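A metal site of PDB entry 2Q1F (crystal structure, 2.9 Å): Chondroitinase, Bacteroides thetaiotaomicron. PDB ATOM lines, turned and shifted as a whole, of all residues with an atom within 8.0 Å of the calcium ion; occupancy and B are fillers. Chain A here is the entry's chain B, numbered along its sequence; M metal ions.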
ATOM      1  N   ALA A  14       5.269  -3.555  22.113  1.00  0.00           N
ATOM      2  CA  ALA A  14       4.823  -4.779  21.384  1.00  0.00           C
ATOM      3  C   ALA A  14       3.555  -4.539  20.576  1.00  0.00           C
ATOM      4  O   ALA A  14       2.680  -3.779  20.992  1.00  0.00           O
ATOM      5  CB  ALA A  14       4.622  -5.931  22.367  1.00  0.00           C
ATOM      6  N   GLN A  15       3.465  -5.166  19.413  1.00  0.00           N
ATOM      7  CA  GLN A  15       2.273  -5.069  18.572  1.00  0.00           C
ATOM      8  C   GLN A  15       1.234  -6.088  19.021  1.00  0.00           C
ATOM      9  O   GLN A  15       1.564  -7.245  19.307  1.00  0.00           O
ATOM     10  CB  GLN A  15       2.605  -5.205  17.083  1.00  0.00           C
ATOM     11  CG  GLN A  15       3.409  -6.449  16.667  1.00  0.00           C
ATOM     12  CD  GLN A  15       2.598  -7.458  15.872  1.00  0.00           C
ATOM     13  OE1 GLN A  15       1.815  -7.091  14.995  1.00  0.00           O
ATOM     14  NE2 GLN A  15       2.784  -8.736  16.184  1.00  0.00           N
ATOM     15  N   MET A  22      -1.384 -10.166   9.062  1.00  0.00           N
ATOM     16  CA  MET A  22      -1.215  -8.904   9.779  1.00  0.00           C
ATOM     17  C   MET A  22       0.160  -8.294   9.483  1.00  0.00           C
ATOM     18  O   MET A  22       1.189  -8.897   9.798  1.00  0.00           O
ATOM     19  CB  MET A  22      -1.390  -9.148  11.288  1.00  0.00           C
ATOM     20  CG  MET A  22      -1.031  -7.995  12.226  1.00  0.00           C
ATOM     21  SD  MET A  22      -2.442  -6.669  12.485  1.00  0.00           S
ATOM     22  CE  MET A  22      -1.912  -5.424  11.097  1.00  0.00           C
ATOM     23  N   PHE A  23       0.161  -7.120   8.862  1.00  0.00           N
ATOM     24  CA  PHE A  23       1.391  -6.388   8.604  1.00  0.00           C
ATOM     25  C   PHE A  23       1.495  -5.126   9.458  1.00  0.00           C
ATOM     26  O   PHE A  23       0.686  -4.198   9.323  1.00  0.00           O
ATOM     27  CB  PHE A  23       1.567  -6.083   7.112  1.00  0.00           C
ATOM     28  CG  PHE A  23       2.081  -7.249   6.322  1.00  0.00           C
ATOM     29  CD1 PHE A  23       3.415  -7.640   6.405  1.00  0.00           C
ATOM     30  CD2 PHE A  23       1.226  -7.978   5.502  1.00  0.00           C
ATOM     31  CE1 PHE A  23       3.896  -8.724   5.690  1.00  0.00           C
ATOM     32  CE2 PHE A  23       1.692  -9.069   4.768  1.00  0.00           C
ATOM     33  CZ  PHE A  23       3.034  -9.441   4.865  1.00  0.00           C
ATOM     34  N   SER A  24       2.485  -5.122  10.348  1.00  0.00           N
ATOM     35  CA  SER A  24       2.681  -4.050  11.310  1.00  0.00           C
ATOM     36  C   SER A  24       4.083  -3.432  11.222  1.00  0.00           C
ATOM     37  O   SER A  24       4.341  -2.404  11.862  1.00  0.00           O
ATOM     38  CB  SER A  24       2.402  -4.569  12.733  1.00  0.00           C
ATOM     39  OG  SER A  24       2.589  -3.555  13.694  1.00  0.00           O
ATOM     40  N   PHE A  25       4.951  -4.068  10.440  1.00  0.00           N
ATOM     41  CA  PHE A  25       6.303  -3.555  10.117  1.00  0.00           C
ATOM     42  C   PHE A  25       7.181  -3.281  11.349  1.00  0.00           C
ATOM     43  O   PHE A  25       7.878  -2.266  11.406  1.00  0.00           O
ATOM     44  CB  PHE A  25       6.229  -2.331   9.200  1.00  0.00           C
ATOM     45  CG  PHE A  25       5.118  -2.397   8.191  1.00  0.00           C
ATOM     46  CD1 PHE A  25       5.177  -3.295   7.128  1.00  0.00           C
ATOM     47  CD2 PHE A  25       4.009  -1.574   8.304  1.00  0.00           C
ATOM     48  CE1 PHE A  25       4.136  -3.375   6.196  1.00  0.00           C
ATOM     49  CE2 PHE A  25       2.971  -1.632   7.376  1.00  0.00           C
ATOM     50  CZ  PHE A  25       3.037  -2.541   6.318  1.00  0.00           C
ATOM     51  N   GLU A  26       7.155  -4.209  12.297  1.00  0.00           N
ATOM     52  CA  GLU A  26       7.893  -4.064  13.551  1.00  0.00           C
ATOM     53  C   GLU A  26       9.314  -4.630  13.471  1.00  0.00           C
ATOM     54  O   GLU A  26      10.084  -4.548  14.424  1.00  0.00           O
ATOM     55  CB  GLU A  26       7.115  -4.709  14.692  1.00  0.00           C
ATOM     56  CG  GLU A  26       7.331  -4.083  16.070  1.00  0.00           C
ATOM     57  CD  GLU A  26       6.861  -2.637  16.168  1.00  0.00           C
ATOM     58  OE1 GLU A  26       5.975  -2.226  15.380  1.00  0.00           O
ATOM     59  OE2 GLU A  26       7.368  -1.911  17.047  1.00  0.00           O
ATOM     60  N   GLU A  27       9.654  -5.202  12.314  1.00  0.00           N
ATOM     61  CA  GLU A  27      10.976  -5.791  12.093  1.00  0.00           C
ATOM     62  C   GLU A  27      11.947  -4.784  11.444  1.00  0.00           C
ATOM     63  O   GLU A  27      11.513  -3.900  10.703  1.00  0.00           O
ATOM     64  CB  GLU A  27      10.884  -7.091  11.256  1.00  0.00           C
ATOM     65  CG  GLU A  27       9.964  -7.033  10.037  1.00  0.00           C
ATOM     66  CD  GLU A  27       8.497  -7.289  10.365  1.00  0.00           C
ATOM     67  OE1 GLU A  27       8.214  -8.154  11.229  1.00  0.00           O
ATOM     68  OE2 GLU A  27       7.625  -6.635   9.755  1.00  0.00           O
ATOM     69  N   ILE A  43      11.263   1.762   6.784  1.00  0.00           N
ATOM     70  CA  ILE A  43      10.650   1.633   8.095  1.00  0.00           C
ATOM     71  C   ILE A  43      10.867   2.940   8.871  1.00  0.00           C
ATOM     72  O   ILE A  43      12.005   3.372   9.059  1.00  0.00           O
ATOM     73  CB  ILE A  43      11.210   0.420   8.898  1.00  0.00           C
ATOM     74  CG1 ILE A  43      10.855  -0.903   8.198  1.00  0.00           C
ATOM     75  CG2 ILE A  43      10.650   0.386  10.313  1.00  0.00           C
ATOM     76  CD1 ILE A  43      11.932  -1.428   7.274  1.00  0.00           C
ATOM     77  N   SER A  44       9.773   3.552   9.297  1.00  0.00           N
ATOM     78  CA  SER A  44       9.799   4.835  10.000  1.00  0.00           C
ATOM     79  C   SER A  44       9.241   4.722  11.415  1.00  0.00           C
ATOM     80  O   SER A  44       8.253   4.019  11.640  1.00  0.00           O
ATOM     81  CB  SER A  44       9.019   5.885   9.215  1.00  0.00           C
ATOM     82  OG  SER A  44       8.772   7.043   9.996  1.00  0.00           O
ATOM     83  N   HIS A  47       5.711   7.842  12.875  1.00  0.00           N
ATOM     84  CA  HIS A  47       4.276   7.618  13.047  1.00  0.00           C
ATOM     85  C   HIS A  47       3.992   6.119  13.162  1.00  0.00           C
ATOM     86  O   HIS A  47       4.644   5.312  12.498  1.00  0.00           O
ATOM     87  CB  HIS A  47       3.488   8.222  11.883  1.00  0.00           C
ATOM     88  CG  HIS A  47       3.918   9.610  11.524  1.00  0.00           C
ATOM     89  ND1 HIS A  47       3.667  10.698  12.333  1.00  0.00           N
ATOM     90  CD2 HIS A  47       4.590  10.090  10.457  1.00  0.00           C
ATOM     91  CE1 HIS A  47       4.164  11.782  11.783  1.00  0.00           C
ATOM     92  NE2 HIS A  47       4.724  11.443  10.629  1.00  0.00           N
ATOM     93  N   TYR A  48       3.029   5.764  14.007  1.00  0.00           N
ATOM     94  CA  TYR A  48       2.652   4.358  14.207  1.00  0.00           C
ATOM     95  C   TYR A  48       1.251   4.199  14.797  1.00  0.00           C
ATOM     96  O   TYR A  48       0.854   4.960  15.689  1.00  0.00           O
ATOM     97  CB  TYR A  48       3.683   3.623  15.084  1.00  0.00           C
ATOM     98  CG  TYR A  48       3.920   4.225  16.456  1.00  0.00           C
ATOM     99  CD1 TYR A  48       4.876   5.220  16.654  1.00  0.00           C
ATOM    100  CD2 TYR A  48       3.199   3.789  17.571  1.00  0.00           C
ATOM    101  CE1 TYR A  48       5.103   5.777  17.914  1.00  0.00           C
ATOM    102  CE2 TYR A  48       3.425   4.331  18.838  1.00  0.00           C
ATOM    103  CZ  TYR A  48       4.368   5.318  18.995  1.00  0.00           C
ATOM    104  OH  TYR A  48       4.588   5.856  20.242  1.00  0.00           O
ATOM    105  N   LYS A  49       0.508   3.221  14.288  1.00  0.00           N
ATOM    106  CA  LYS A  49      -0.832   2.914  14.769  1.00  0.00           C
ATOM    107  C   LYS A  49      -0.836   1.673  15.673  1.00  0.00           C
ATOM    108  O   LYS A  49      -1.748   1.483  16.482  1.00  0.00           O
ATOM    109  CB  LYS A  49      -1.803   2.743  13.601  1.00  0.00           C
ATOM    110  CG  LYS A  49      -3.279   2.732  13.983  1.00  0.00           C
ATOM    111  CD  LYS A  49      -3.747   4.094  14.483  1.00  0.00           C
ATOM    112  CE  LYS A  49      -5.011   3.952  15.309  1.00  0.00           C
ATOM    113  NZ  LYS A  49      -5.645   5.264  15.578  1.00  0.00           N
ATOM    114  N   ASP A  50       0.175   0.820  15.509  1.00  0.00           N
ATOM    115  CA  ASP A  50       0.426  -0.270  16.444  1.00  0.00           C
ATOM    116  C   ASP A  50       1.921  -0.578  16.471  1.00  0.00           C
ATOM    117  O   ASP A  50       2.624  -0.382  15.481  1.00  0.00           O
ATOM    118  CB  ASP A  50      -0.410  -1.526  16.122  1.00  0.00           C
ATOM    119  CG  ASP A  50       0.171  -2.354  14.990  1.00  0.00           C
ATOM    120  OD1 ASP A  50       0.547  -1.790  13.947  1.00  0.00           O
ATOM    121  OD2 ASP A  50       0.236  -3.598  15.143  1.00  0.00           O
ATOM    122  N   GLY A  51       2.395  -1.063  17.619  1.00  0.00           N
ATOM    123  CA  GLY A  51       3.824  -1.255  17.827  1.00  0.00           C
ATOM    124  C   GLY A  51       4.493   0.088  17.993  1.00  0.00           C
ATOM    125  O   GLY A  51       4.034   0.923  18.776  1.00  0.00           O
ATOM    126  N   LYS A  52       5.565   0.301  17.238  1.00  0.00           N
ATOM    127  CA  LYS A  52       6.346   1.540  17.329  1.00  0.00           C
ATOM    128  C   LYS A  52       6.844   2.008  15.965  1.00  0.00           C
ATOM    129  O   LYS A  52       7.592   2.990  15.872  1.00  0.00           O
ATOM    130  CB  LYS A  52       7.520   1.352  18.291  1.00  0.00           C
ATOM    131  CG  LYS A  52       7.250   1.767  19.725  1.00  0.00           C
ATOM    132  CD  LYS A  52       8.026   0.919  20.743  1.00  0.00           C
ATOM    133  CE  LYS A  52       9.530   0.818  20.455  1.00  0.00           C
ATOM    134  NZ  LYS A  52      10.269   2.105  20.616  1.00  0.00           N
ATOM    135  N   HIS A  53       6.432   1.309  14.908  1.00  0.00           N
ATOM    136  CA  HIS A  53       6.911   1.590  13.546  1.00  0.00           C
ATOM    137  C   HIS A  53       5.786   1.555  12.506  1.00  0.00           C
ATOM    138  O   HIS A  53       4.715   1.007  12.760  1.00  0.00           O
ATOM    139  CB  HIS A  53       7.996   0.588  13.151  1.00  0.00           C
ATOM    140  CG  HIS A  53       9.179   0.562  14.086  1.00  0.00           C
ATOM    141  ND1 HIS A  53      10.317   1.296  13.864  1.00  0.00           N
ATOM    142  CD2 HIS A  53       9.383  -0.125  15.230  1.00  0.00           C
ATOM    143  CE1 HIS A  53      11.184   1.072  14.831  1.00  0.00           C
ATOM    144  NE2 HIS A  53      10.645   0.219  15.677  1.00  0.00           N
ATOM    145  N   SER A  54       6.047   2.148  11.344  1.00  0.00           N
ATOM    146  CA  SER A  54       5.148   2.066  10.201  1.00  0.00           C
ATOM    147  C   SER A  54       5.949   2.091   8.892  1.00  0.00           C
ATOM    148  O   SER A  54       7.157   2.349   8.902  1.00  0.00           O
ATOM    149  CB  SER A  54       4.127   3.198  10.208  1.00  0.00           C
ATOM    150  OG  SER A  54       4.747   4.457  10.016  1.00  0.00           O
ATOM    151  N   LEU A  55       5.268   1.811   7.779  1.00  0.00           N
ATOM    152  CA  LEU A  55       5.917   1.789   6.475  1.00  0.00           C
ATOM    153  C   LEU A  55       5.812   3.142   5.785  1.00  0.00           C
ATOM    154  O   LEU A  55       4.719   3.605   5.439  1.00  0.00           O
ATOM    155  CB  LEU A  55       5.325   0.681   5.587  1.00  0.00           C
ATOM    156  CG  LEU A  55       6.110   0.256   4.341  1.00  0.00           C
ATOM    157  CD1 LEU A  55       5.823  -1.188   3.989  1.00  0.00           C
ATOM    158  CD2 LEU A  55       5.824   1.164   3.152  1.00  0.00           C
ATOM    159  N   TRP A 125      -3.761  10.217  11.168  1.00  0.00           N
ATOM    160  CA  TRP A 125      -4.186   8.851  10.884  1.00  0.00           C
ATOM    161  C   TRP A 125      -5.647   8.779  10.454  1.00  0.00           C
ATOM    162  O   TRP A 125      -6.506   9.413  11.068  1.00  0.00           O
ATOM    163  CB  TRP A 125      -3.997   7.978  12.133  1.00  0.00           C
ATOM    164  CG  TRP A 125      -2.592   7.545  12.388  1.00  0.00           C
ATOM    165  CD1 TRP A 125      -1.786   7.958  13.407  1.00  0.00           C
ATOM    166  CD2 TRP A 125      -1.828   6.612  11.619  1.00  0.00           C
ATOM    167  NE1 TRP A 125      -0.557   7.351  13.319  1.00  0.00           N
ATOM    168  CE2 TRP A 125      -0.557   6.513  12.235  1.00  0.00           C
ATOM    169  CE3 TRP A 125      -2.086   5.852  10.467  1.00  0.00           C
ATOM    170  CZ2 TRP A 125       0.446   5.681  11.733  1.00  0.00           C
ATOM    171  CZ3 TRP A 125      -1.081   5.027   9.978  1.00  0.00           C
ATOM    172  CH2 TRP A 125       0.166   4.946  10.611  1.00  0.00           C
ATOM    173  N   ILE A 160       2.006   3.849   6.145  1.00  0.00           N
ATOM    174  CA  ILE A 160       1.037   2.758   6.261  1.00  0.00           C
ATOM    175  C   ILE A 160       1.363   1.864   7.446  1.00  0.00           C
ATOM    176  O   ILE A 160       2.516   1.457   7.650  1.00  0.00           O
ATOM    177  CB  ILE A 160       0.954   1.901   4.958  1.00  0.00           C
ATOM    178  CG1 ILE A 160       0.738   2.800   3.730  1.00  0.00           C
ATOM    179  CG2 ILE A 160      -0.162   0.864   5.058  1.00  0.00           C
ATOM    180  CD1 ILE A 160       1.032   2.134   2.397  1.00  0.00           C
ATOM    181  N   ASP A 161       0.335   1.565   8.246  1.00  0.00           N
ATOM    182  CA  ASP A 161       0.453   0.639   9.365  1.00  0.00           C
ATOM    183  C   ASP A 161      -0.881  -0.059   9.604  1.00  0.00           C
ATOM    184  O   ASP A 161      -1.903   0.358   9.048  1.00  0.00           O
ATOM    185  CB  ASP A 161       0.925   1.361  10.642  1.00  0.00           C
ATOM    186  CG  ASP A 161       1.575   0.424  11.651  1.00  0.00           C
ATOM    187  OD1 ASP A 161       1.683   0.822  12.833  1.00  0.00           O
ATOM    188  OD2 ASP A 161       1.983  -0.697  11.285  1.00  0.00           O
ATOM    189  N   HIS A 162      -0.865  -1.117  10.412  1.00  0.00           N
ATOM    190  CA  HIS A 162      -2.050  -1.897  10.760  1.00  0.00           C
ATOM    191  C   HIS A 162      -2.773  -2.401   9.511  1.00  0.00           C
ATOM    192  O   HIS A 162      -3.959  -2.128   9.307  1.00  0.00           O
ATOM    193  CB  HIS A 162      -3.001  -1.087  11.657  1.00  0.00           C
ATOM    194  CG  HIS A 162      -3.889  -1.909  12.537  1.00  0.00           C
ATOM    195  ND1 HIS A 162      -3.859  -1.821  13.911  1.00  0.00           N
ATOM    196  CD2 HIS A 162      -4.815  -2.850  12.234  1.00  0.00           C
ATOM    197  CE1 HIS A 162      -4.736  -2.661  14.422  1.00  0.00           C
ATOM    198  NE2 HIS A 162      -5.326  -3.303  13.424  1.00  0.00           N
HETATM  199 CA    CA M   1       4.111  -1.070  13.806  1.00  0.00          CA
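The side-chain carboxylate (OD1) of Asp 161 is in hydrogen-bond range of the backbone NH (N) of Lys 49 (3.0 Å). The backbone NH of Asp 50 sits at hydrogen-bond distance from the side-chain carboxylate of Asp 161, 3.1 Å away. OE2 of Glu 26 sits at hydrogen-bond distance from N of Lys 52 (2.9 Å).
Lys 52 touches the calcium ion (N to CA, 3.97 Å). Asp 161 touches the calcium ion (OD1 to CA, 3.2 Å). Six residues have an atom within 4 Å of the calcium ion: Ser 24, Glu 26, Asp 50, Lys 52, His 53 and Asp 161. Along chain A the residues within 4 Å of the calcium ion span positions 24 to 161. The nearest printed residue that does not touch the calcium ion is Gly 51 (4.04 Å).
The calcium ion is bound by the backbone carbonyl oxygen (O) of Asp 50 (2.3 Å), the backbone carbonyl oxygen (O) of Ser 24 (2.4 Å), the backbone carbonyl oxygen (O) of His 53 (2.4 Å) and the side-chain carboxylate (OE1) of Glu 26 (2.7 Å). The calcium ion has four donor atoms within binding distance. Slightly farther from the calcium ion lies the side-chain hydroxyl (OG) of Ser 24 (2.9 Å).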
